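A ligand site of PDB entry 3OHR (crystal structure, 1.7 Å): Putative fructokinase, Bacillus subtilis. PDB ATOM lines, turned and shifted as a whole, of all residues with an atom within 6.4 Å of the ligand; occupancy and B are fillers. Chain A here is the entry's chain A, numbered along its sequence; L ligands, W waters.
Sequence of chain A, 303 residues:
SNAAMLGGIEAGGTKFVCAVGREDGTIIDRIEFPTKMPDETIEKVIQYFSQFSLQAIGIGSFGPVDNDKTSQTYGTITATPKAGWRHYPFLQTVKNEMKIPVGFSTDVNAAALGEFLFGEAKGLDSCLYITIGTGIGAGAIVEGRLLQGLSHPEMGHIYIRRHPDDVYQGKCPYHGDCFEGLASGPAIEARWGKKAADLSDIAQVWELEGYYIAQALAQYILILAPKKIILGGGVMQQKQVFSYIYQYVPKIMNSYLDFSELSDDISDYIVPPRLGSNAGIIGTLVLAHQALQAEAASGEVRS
N of Gly 234 sits at hydrogen-bond distance from O of Ile 132, 3.3 Å away. N of Gly 185 sits at hydrogen-bond distance from O of Gly 133. O of Gly 233 lies within hydrogen-bond range of NE2 of Gln 237. The backbone NH (N) of Val 235 is in hydrogen-bond range of the backbone carbonyl oxygen (O) of Ile 132 (3.0 Å).
O9 of the ligand lies close to N of Pro 186 (3.3 Å). Gly 133 touches the ligand. C of Gly 185 touches O9 of the ligand, at 3.1 Å. Ala 196 touches the ligand (CB to N5, 3.3 Å). Ala 197 touches the ligand. CA of Gly 233 touches O5 of the ligand (3.7 Å). Val 235 touches the ligand (CA to N5, 3.8 Å). Gln 237 touches the ligand. Hydrophobic or aromatic side chains that line the ligand: Pro 186, Ala 196, Ala 197 and Val 235. The nearest printed residue that does not touch the ligand is Lys 195 (4.3 Å).
O3 of the ligand sits at hydrogen-bond distance from N of Thr 134. OG1 of Thr 134 is in hydrogen-bond range of O2 of the ligand (2.6 Å). The backbone NH of Gly 234 is in hydrogen-bond range of an oxygen (O5) of the ligand, at 2.8 Å. A nitrogen (N4) of the ligand sits close to the side-chain amide oxygen (OE1) of Gln 238 (3.2 Å).
Water W14 bridges O9 of the ligand (2.6 Å) and OE2 of Glu 189 (2.8 Å). Water W13 lies within hydrogen-bond range of an oxygen (O3) of the ligand (2.6 Å), the backbone NH of Gly 135 (2.9 Å) and the backbone NH of Thr 134 (3.4 Å). Water W5 lies within hydrogen-bond range of the side-chain hydroxyl of Thr 131 (2.5 Å) and an oxygen (O5) of the ligand (2.6 Å). Water W9 bridges an oxygen (O2) of the ligand (2.7 Å) and the side-chain hydroxyl (OG1) of Thr 14 (2.9 Å). Water W8 lies within hydrogen-bond range of an oxygen (O10) of the ligand, the backbone carbonyl oxygen of Gly 185 and the backbone NH of Ala 196. Water W7 lies within hydrogen-bond range of the backbone NH (N) of Ala 197, an oxygen (O10) of the ligand and the backbone NH (N) of Ala 196.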
ATOM      1  N   GLY A  12     -24.346 -22.850  42.508  1.00  0.00           N
ATOM      2  CA  GLY A  12     -24.480 -22.875  41.070  1.00  0.00           C
ATOM      3  C   GLY A  12     -25.816 -22.408  40.601  1.00  0.00           C
ATOM      4  O   GLY A  12     -26.784 -22.220  41.369  1.00  0.00           O
ATOM      5  N   GLY A  13     -25.884 -22.161  39.299  1.00  0.00           N
ATOM      6  CA  GLY A  13     -27.078 -21.643  38.732  1.00  0.00           C
ATOM      7  C   GLY A  13     -28.202 -22.635  38.820  1.00  0.00           C
ATOM      8  O   GLY A  13     -29.365 -22.224  38.883  1.00  0.00           O
ATOM      9  N   THR A  14     -27.877 -23.934  38.776  1.00  0.00           N
ATOM     10  CA  THR A  14     -28.899 -24.988  38.762  1.00  0.00           C
ATOM     11  C   THR A  14     -29.075 -25.644  40.137  1.00  0.00           C
ATOM     12  O   THR A  14     -30.192 -25.957  40.519  1.00  0.00           O
ATOM     13  CB  THR A  14     -28.519 -26.058  37.733  1.00  0.00           C
ATOM     14  OG1 THR A  14     -28.384 -25.423  36.450  1.00  0.00           O
ATOM     15  CG2 THR A  14     -29.560 -27.167  37.650  1.00  0.00           C
ATOM     16  N   ASP A 107     -16.863 -19.909  41.980  1.00  0.00           N
ATOM     17  CA  ASP A 107     -16.853 -21.367  42.030  1.00  0.00           C
ATOM     18  C   ASP A 107     -15.605 -21.951  41.388  1.00  0.00           C
ATOM     19  O   ASP A 107     -15.011 -22.908  41.909  1.00  0.00           O
ATOM     20  CB  ASP A 107     -18.115 -21.974  41.393  1.00  0.00           C
ATOM     21  CG  ASP A 107     -18.484 -21.387  40.033  1.00  0.00           C
ATOM     22  OD1 ASP A 107     -17.795 -20.495  39.472  1.00  0.00           O
ATOM     23  OD2 ASP A 107     -19.506 -21.898  39.470  1.00  0.00           O
ATOM     24  N   THR A 131     -13.370 -24.790  33.899  1.00  0.00           N
ATOM     25  CA  THR A 131     -14.513 -25.707  33.734  1.00  0.00           C
ATOM     26  C   THR A 131     -15.187 -25.451  32.392  1.00  0.00           C
ATOM     27  O   THR A 131     -15.349 -24.271  31.968  1.00  0.00           O
ATOM     28  CB  THR A 131     -15.528 -25.552  34.886  1.00  0.00           C
ATOM     29  OG1 THR A 131     -16.470 -26.635  34.817  1.00  0.00           O
ATOM     30  CG2 THR A 131     -16.331 -24.266  34.822  1.00  0.00           C
ATOM     31  N   ILE A 132     -15.619 -26.524  31.734  1.00  0.00           N
ATOM     32  CA  ILE A 132     -16.350 -26.438  30.499  1.00  0.00           C
ATOM     33  C   ILE A 132     -17.652 -27.230  30.745  1.00  0.00           C
ATOM     34  O   ILE A 132     -17.667 -28.462  30.801  1.00  0.00           O
ATOM     35  CB  ILE A 132     -15.564 -26.935  29.325  1.00  0.00           C
ATOM     36  CG1 ILE A 132     -14.283 -26.072  29.177  1.00  0.00           C
ATOM     37  CG2 ILE A 132     -16.401 -26.852  28.028  1.00  0.00           C
ATOM     38  CD1 ILE A 132     -13.426 -26.518  28.108  1.00  0.00           C
ATOM     39  N   GLY A 133     -18.739 -26.468  30.951  1.00  0.00           N
ATOM     40  CA  GLY A 133     -20.052 -27.033  31.266  1.00  0.00           C
ATOM     41  C   GLY A 133     -21.146 -26.166  30.696  1.00  0.00           C
ATOM     42  O   GLY A 133     -21.144 -25.890  29.527  1.00  0.00           O
ATOM     43  N   THR A 134     -22.099 -25.731  31.543  1.00  0.00           N
ATOM     44  CA  THR A 134     -23.149 -24.837  31.139  1.00  0.00           C
ATOM     45  C   THR A 134     -22.535 -23.529  30.651  1.00  0.00           C
ATOM     46  O   THR A 134     -23.004 -22.984  29.663  1.00  0.00           O
ATOM     47  CB  THR A 134     -24.165 -24.628  32.271  1.00  0.00           C
ATOM     48  OG1 THR A 134     -24.760 -25.886  32.599  1.00  0.00           O
ATOM     49  CG2 THR A 134     -25.260 -23.589  31.846  1.00  0.00           C
ATOM     50  N   GLY A 135     -21.488 -23.060  31.333  1.00  0.00           N
ATOM     51  CA  GLY A 135     -20.673 -21.965  30.863  1.00  0.00           C
ATOM     52  C   GLY A 135     -19.223 -22.409  30.850  1.00  0.00           C
ATOM     53  O   GLY A 135     -18.906 -23.555  31.166  1.00  0.00           O
ATOM     54  N   SER A 184     -19.202 -24.288  25.024  1.00  0.00           N
ATOM     55  CA  SER A 184     -19.840 -24.754  26.205  1.00  0.00           C
ATOM     56  C   SER A 184     -20.661 -25.984  25.830  1.00  0.00           C
ATOM     57  O   SER A 184     -20.924 -26.227  24.658  1.00  0.00           O
ATOM     58  CB  SER A 184     -20.800 -23.679  26.769  1.00  0.00           C
ATOM     59  OG  SER A 184     -21.914 -23.484  25.885  1.00  0.00           O
ATOM     60  N   GLY A 185     -21.078 -26.697  26.854  1.00  0.00           N
ATOM     61  CA  GLY A 185     -22.073 -27.773  26.701  1.00  0.00           C
ATOM     62  C   GLY A 185     -23.300 -27.413  25.907  1.00  0.00           C
ATOM     63  O   GLY A 185     -23.656 -28.137  24.963  1.00  0.00           O
ATOM     64  N   PRO A 186     -23.982 -26.316  26.280  1.00  0.00           N
ATOM     65  CA  PRO A 186     -25.138 -25.888  25.520  1.00  0.00           C
ATOM     66  C   PRO A 186     -24.839 -25.470  24.088  1.00  0.00           C
ATOM     67  O   PRO A 186     -25.668 -25.619  23.236  1.00  0.00           O
ATOM     68  CB  PRO A 186     -25.707 -24.737  26.357  1.00  0.00           C
ATOM     69  CG  PRO A 186     -25.230 -25.096  27.804  1.00  0.00           C
ATOM     70  CD  PRO A 186     -23.849 -25.604  27.557  1.00  0.00           C
ATOM     71  N   ALA A 187     -23.651 -24.945  23.813  1.00  0.00           N
ATOM     72  CA  ALA A 187     -23.283 -24.580  22.448  1.00  0.00           C
ATOM     73  C   ALA A 187     -23.122 -25.820  21.578  1.00  0.00           C
ATOM     74  O   ALA A 187     -23.509 -25.821  20.413  1.00  0.00           O
ATOM     75  CB  ALA A 187     -21.953 -23.785  22.463  1.00  0.00           C
ATOM     76  N   ILE A 188     -22.537 -26.849  22.157  1.00  0.00           N
ATOM     77  CA  ILE A 188     -22.364 -28.120  21.499  1.00  0.00           C
ATOM     78  C   ILE A 188     -23.741 -28.663  21.144  1.00  0.00           C
ATOM     79  O   ILE A 188     -23.946 -29.102  20.010  1.00  0.00           O
ATOM     80  CB  ILE A 188     -21.574 -29.145  22.348  1.00  0.00           C
ATOM     81  CG1 ILE A 188     -20.124 -28.733  22.532  1.00  0.00           C
ATOM     82  CG2 ILE A 188     -21.685 -30.583  21.765  1.00  0.00           C
ATOM     83  CD1 ILE A 188     -19.360 -29.605  23.515  1.00  0.00           C
ATOM     84  N   GLU A 189     -24.650 -28.670  22.115  1.00  0.00           N
ATOM     85  CA  GLU A 189     -26.020 -29.156  21.910  1.00  0.00           C
ATOM     86  C   GLU A 189     -26.755 -28.353  20.836  1.00  0.00           C
ATOM     87  O   GLU A 189     -27.444 -28.920  19.979  1.00  0.00           O
ATOM     88  CB  GLU A 189     -26.768 -29.170  23.243  1.00  0.00           C
ATOM     89  CG  GLU A 189     -28.221 -29.575  23.108  1.00  0.00           C
ATOM     90  CD  GLU A 189     -28.925 -29.933  24.394  1.00  0.00           C
ATOM     91  OE1 GLU A 189     -30.107 -30.343  24.270  1.00  0.00           O
ATOM     92  OE2 GLU A 189     -28.359 -29.859  25.505  1.00  0.00           O
ATOM     93  N   LYS A 195     -27.637 -33.483  22.990  1.00  0.00           N
ATOM     94  CA  LYS A 195     -26.772 -33.178  24.096  1.00  0.00           C
ATOM     95  C   LYS A 195     -25.430 -33.803  23.946  1.00  0.00           C
ATOM     96  O   LYS A 195     -25.276 -34.816  23.324  1.00  0.00           O
ATOM     97  CB  LYS A 195     -27.390 -33.497  25.441  1.00  0.00           C
ATOM     98  CG  LYS A 195     -27.838 -34.849  25.624  1.00  0.00           C
ATOM     99  CD  LYS A 195     -28.674 -34.968  26.911  1.00  0.00           C
ATOM    100  CE  LYS A 195     -28.261 -36.224  27.648  1.00  0.00           C
ATOM    101  NZ  LYS A 195     -28.914 -36.468  28.956  1.00  0.00           N
ATOM    102  N   ALA A 196     -24.434 -33.164  24.523  1.00  0.00           N
ATOM    103  CA  ALA A 196     -23.049 -33.496  24.250  1.00  0.00           C
ATOM    104  C   ALA A 196     -22.733 -34.944  24.590  1.00  0.00           C
ATOM    105  O   ALA A 196     -22.049 -35.617  23.830  1.00  0.00           O
ATOM    106  CB  ALA A 196     -22.101 -32.516  25.045  1.00  0.00           C
ATOM    107  N   ALA A 197     -23.242 -35.443  25.724  1.00  0.00           N
ATOM    108  CA  ALA A 197     -23.014 -36.830  26.100  1.00  0.00           C
ATOM    109  C   ALA A 197     -23.494 -37.817  25.021  1.00  0.00           C
ATOM    110  O   ALA A 197     -22.905 -38.878  24.848  1.00  0.00           O
ATOM    111  CB  ALA A 197     -23.662 -37.159  27.421  1.00  0.00           C
ATOM    112  N   ASP A 198     -24.539 -37.445  24.294  1.00  0.00           N
ATOM    113  CA  ASP A 198     -25.130 -38.315  23.240  1.00  0.00           C
ATOM    114  C   ASP A 198     -24.398 -38.189  21.897  1.00  0.00           C
ATOM    115  O   ASP A 198     -24.823 -38.787  20.922  1.00  0.00           O
ATOM    116  CB  ASP A 198     -26.608 -37.984  23.019  1.00  0.00           C
ATOM    117  CG  ASP A 198     -27.485 -38.296  24.238  1.00  0.00           C
ATOM    118  OD1 ASP A 198     -28.630 -37.844  24.263  1.00  0.00           O
ATOM    119  OD2 ASP A 198     -27.055 -39.001  25.158  1.00  0.00           O
ATOM    120  N   TRP A 206     -15.830 -33.577  18.729  1.00  0.00           N
ATOM    121  CA  TRP A 206     -14.755 -33.449  19.695  1.00  0.00           C
ATOM    122  C   TRP A 206     -13.495 -32.861  19.074  1.00  0.00           C
ATOM    123  O   TRP A 206     -12.710 -32.204  19.775  1.00  0.00           O
ATOM    124  CB  TRP A 206     -14.510 -34.787  20.376  1.00  0.00           C
ATOM    125  CG  TRP A 206     -15.820 -35.304  20.784  1.00  0.00           C
ATOM    126  CD1 TRP A 206     -16.496 -36.369  20.212  1.00  0.00           C
ATOM    127  CD2 TRP A 206     -16.730 -34.696  21.706  1.00  0.00           C
ATOM    128  NE1 TRP A 206     -17.737 -36.486  20.801  1.00  0.00           N
ATOM    129  CE2 TRP A 206     -17.896 -35.473  21.710  1.00  0.00           C
ATOM    130  CE3 TRP A 206     -16.657 -33.580  22.547  1.00  0.00           C
ATOM    131  CZ2 TRP A 206     -18.981 -35.171  22.511  1.00  0.00           C
ATOM    132  CZ3 TRP A 206     -17.721 -33.290  23.344  1.00  0.00           C
ATOM    133  CH2 TRP A 206     -18.880 -34.074  23.326  1.00  0.00           C
ATOM    134  N   GLY A 232     -11.857 -29.279  33.814  1.00  0.00           N
ATOM    135  CA  GLY A 232     -12.998 -29.991  34.387  1.00  0.00           C
ATOM    136  C   GLY A 232     -14.308 -29.546  33.779  1.00  0.00           C
ATOM    137  O   GLY A 232     -14.335 -28.873  32.749  1.00  0.00           O
ATOM    138  N   GLY A 233     -15.415 -30.021  34.379  1.00  0.00           N
ATOM    139  CA  GLY A 233     -16.737 -29.718  33.892  1.00  0.00           C
ATOM    140  C   GLY A 233     -17.341 -30.893  33.143  1.00  0.00           C
ATOM    141  O   GLY A 233     -16.600 -31.834  32.699  1.00  0.00           O
ATOM    142  N   GLY A 234     -18.658 -30.800  32.917  1.00  0.00           N
ATOM    143  CA  GLY A 234     -19.397 -31.836  32.197  1.00  0.00           C
ATOM    144  C   GLY A 234     -18.818 -32.251  30.869  1.00  0.00           C
ATOM    145  O   GLY A 234     -18.702 -33.471  30.542  1.00  0.00           O
ATOM    146  N   VAL A 235     -18.456 -31.262  30.050  1.00  0.00           N
ATOM    147  CA  VAL A 235     -18.015 -31.547  28.709  1.00  0.00           C
ATOM    148  C   VAL A 235     -16.708 -32.340  28.769  1.00  0.00           C
ATOM    149  O   VAL A 235     -16.489 -33.231  27.967  1.00  0.00           O
ATOM    150  CB  VAL A 235     -17.879 -30.228  27.906  1.00  0.00           C
ATOM    151  CG1 VAL A 235     -17.135 -30.407  26.557  1.00  0.00           C
ATOM    152  CG2 VAL A 235     -19.284 -29.560  27.723  1.00  0.00           C
ATOM    153  N   MET A 236     -15.865 -32.036  29.771  1.00  0.00           N
ATOM    154  CA  MET A 236     -14.571 -32.720  29.885  1.00  0.00           C
ATOM    155  C   MET A 236     -14.678 -34.119  30.454  1.00  0.00           C
ATOM    156  O   MET A 236     -13.680 -34.800  30.590  1.00  0.00           O
ATOM    157  CB  MET A 236     -13.568 -31.879  30.685  1.00  0.00           C
ATOM    158  CG  MET A 236     -13.292 -30.500  30.113  1.00  0.00           C
ATOM    159  SD  MET A 236     -12.646 -30.532  28.266  1.00  0.00           S
ATOM    160  CE  MET A 236     -11.310 -31.981  28.507  1.00  0.00           C
ATOM    161  N   GLN A 237     -15.885 -34.598  30.718  1.00  0.00           N
ATOM    162  CA  GLN A 237     -16.039 -36.032  30.915  1.00  0.00           C
ATOM    163  C   GLN A 237     -15.795 -36.802  29.603  1.00  0.00           C
ATOM    164  O   GLN A 237     -15.603 -38.028  29.629  1.00  0.00           O
ATOM    165  CB  GLN A 237     -17.450 -36.334  31.526  1.00  0.00           C
ATOM    166  CG  GLN A 237     -17.739 -35.549  32.838  1.00  0.00           C
ATOM    167  CD  GLN A 237     -16.553 -35.499  33.828  1.00  0.00           C
ATOM    168  OE1 GLN A 237     -16.180 -36.501  34.396  1.00  0.00           O
ATOM    169  NE2 GLN A 237     -15.960 -34.300  34.022  1.00  0.00           N
ATOM    170  N   GLN A 238     -15.869 -36.119  28.479  1.00  0.00           N
ATOM    171  CA  GLN A 238     -15.527 -36.714  27.205  1.00  0.00           C
ATOM    172  C   GLN A 238     -14.012 -36.675  27.082  1.00  0.00           C
ATOM    173  O   GLN A 238     -13.469 -35.776  26.536  1.00  0.00           O
ATOM    174  CB  GLN A 238     -16.187 -36.025  26.018  1.00  0.00           C
ATOM    175  CG  GLN A 238     -17.664 -36.029  26.015  1.00  0.00           C
ATOM    176  CD  GLN A 238     -18.260 -37.419  25.919  1.00  0.00           C
ATOM    177  OE1 GLN A 238     -19.144 -37.753  26.646  1.00  0.00           O
ATOM    178  NE2 GLN A 238     -17.774 -38.189  25.015  1.00  0.00           N
HETATM  179  P1  LIG L   1     -22.766 -26.864  35.372  1.00  0.00           P
HETATM  180  O1  LIG L   1     -22.360 -26.789  36.814  1.00  0.00           O
HETATM  181  O2  LIG L   1     -24.232 -26.439  35.115  1.00  0.00           O
HETATM  182  O3  LIG L   1     -21.791 -26.185  34.344  1.00  0.00           O
HETATM  183  P2  LIG L   1     -21.813 -29.317  34.089  1.00  0.00           P
HETATM  184  O4  LIG L   1     -22.353 -30.691  34.379  1.00  0.00           O
HETATM  185  O5  LIG L   1     -20.331 -29.087  34.424  1.00  0.00           O
HETATM  186  O6  LIG L   1     -22.710 -28.418  35.042  1.00  0.00           O
HETATM  187  O7  LIG L   1     -22.136 -28.885  32.735  1.00  0.00           O
HETATM  188  C1  LIG L   1     -23.362 -29.096  31.991  1.00  0.00           C
HETATM  189  C2  LIG L   1     -23.176 -29.105  30.526  1.00  0.00           C
HETATM  190  O8  LIG L   1     -22.262 -30.113  30.142  1.00  0.00           O
HETATM  191  C3  LIG L   1     -24.478 -29.395  29.728  1.00  0.00           C
HETATM  192  O9  LIG L   1     -24.466 -28.766  28.470  1.00  0.00           O
HETATM  193  C4  LIG L   1     -24.420 -30.901  29.656  1.00  0.00           C
HETATM  194  O10 LIG L   1     -25.215 -31.415  28.530  1.00  0.00           O
HETATM  195  C5  LIG L   1     -22.966 -31.196  29.380  1.00  0.00           C
HETATM  196  N1  LIG L   1     -22.581 -32.505  29.941  1.00  0.00           N
HETATM  197  C6  LIG L   1     -22.868 -32.977  31.150  1.00  0.00           C
HETATM  198  N2  LIG L   1     -22.363 -34.190  31.309  1.00  0.00           N
HETATM  199  C7  LIG L   1     -21.728 -34.490  30.160  1.00  0.00           C
HETATM  200  C8  LIG L   1     -20.987 -35.582  29.728  1.00  0.00           C
HETATM  201  N3  LIG L   1     -20.832 -36.642  30.541  1.00  0.00           N
HETATM  202  N4  LIG L   1     -20.433 -35.531  28.489  1.00  0.00           N
HETATM  203  C9  LIG L   1     -20.570 -34.445  27.709  1.00  0.00           C
HETATM  204  N5  LIG L   1     -21.288 -33.373  28.087  1.00  0.00           N
HETATM  205  C10 LIG L   1     -21.826 -33.386  29.325  1.00  0.00           C
HETATM  206  O   HOH W   1     -26.094 -28.161  35.331  1.00  0.00           O
HETATM  207  O   HOH W   2     -25.279 -30.616  34.848  1.00  0.00           O
HETATM  208  O   HOH W   3     -27.775 -31.546  29.335  1.00  0.00           O
HETATM  209  O   HOH W   4     -19.542 -39.294  29.793  1.00  0.00           O
HETATM  210  O   HOH W   5     -18.991 -26.843  34.779  1.00  0.00           O
HETATM  211  O   HOH W   6     -22.786 -24.898  38.426  1.00  0.00           O
HETATM  212  O   HOH W   7     -24.734 -34.192  27.770  1.00  0.00           O
HETATM  213  O   HOH W   8     -24.746 -30.609  25.855  1.00  0.00           O
HETATM  214  O   HOH W   9     -25.722 -24.402  36.049  1.00  0.00           O
HETATM  215  O   HOH W  10     -21.015 -33.030  35.093  1.00  0.00           O
HETATM  216  O   HOH W  11     -19.790 -26.557  37.539  1.00  0.00           O
HETATM  217  O   HOH W  12     -23.280 -28.514  38.527  1.00  0.00           O
HETATM  218  O   HOH W  13     -20.808 -23.828  34.059  1.00  0.00           O
HETATM  219  O   HOH W  14     -26.760 -28.521  27.339  1.00  0.00           O
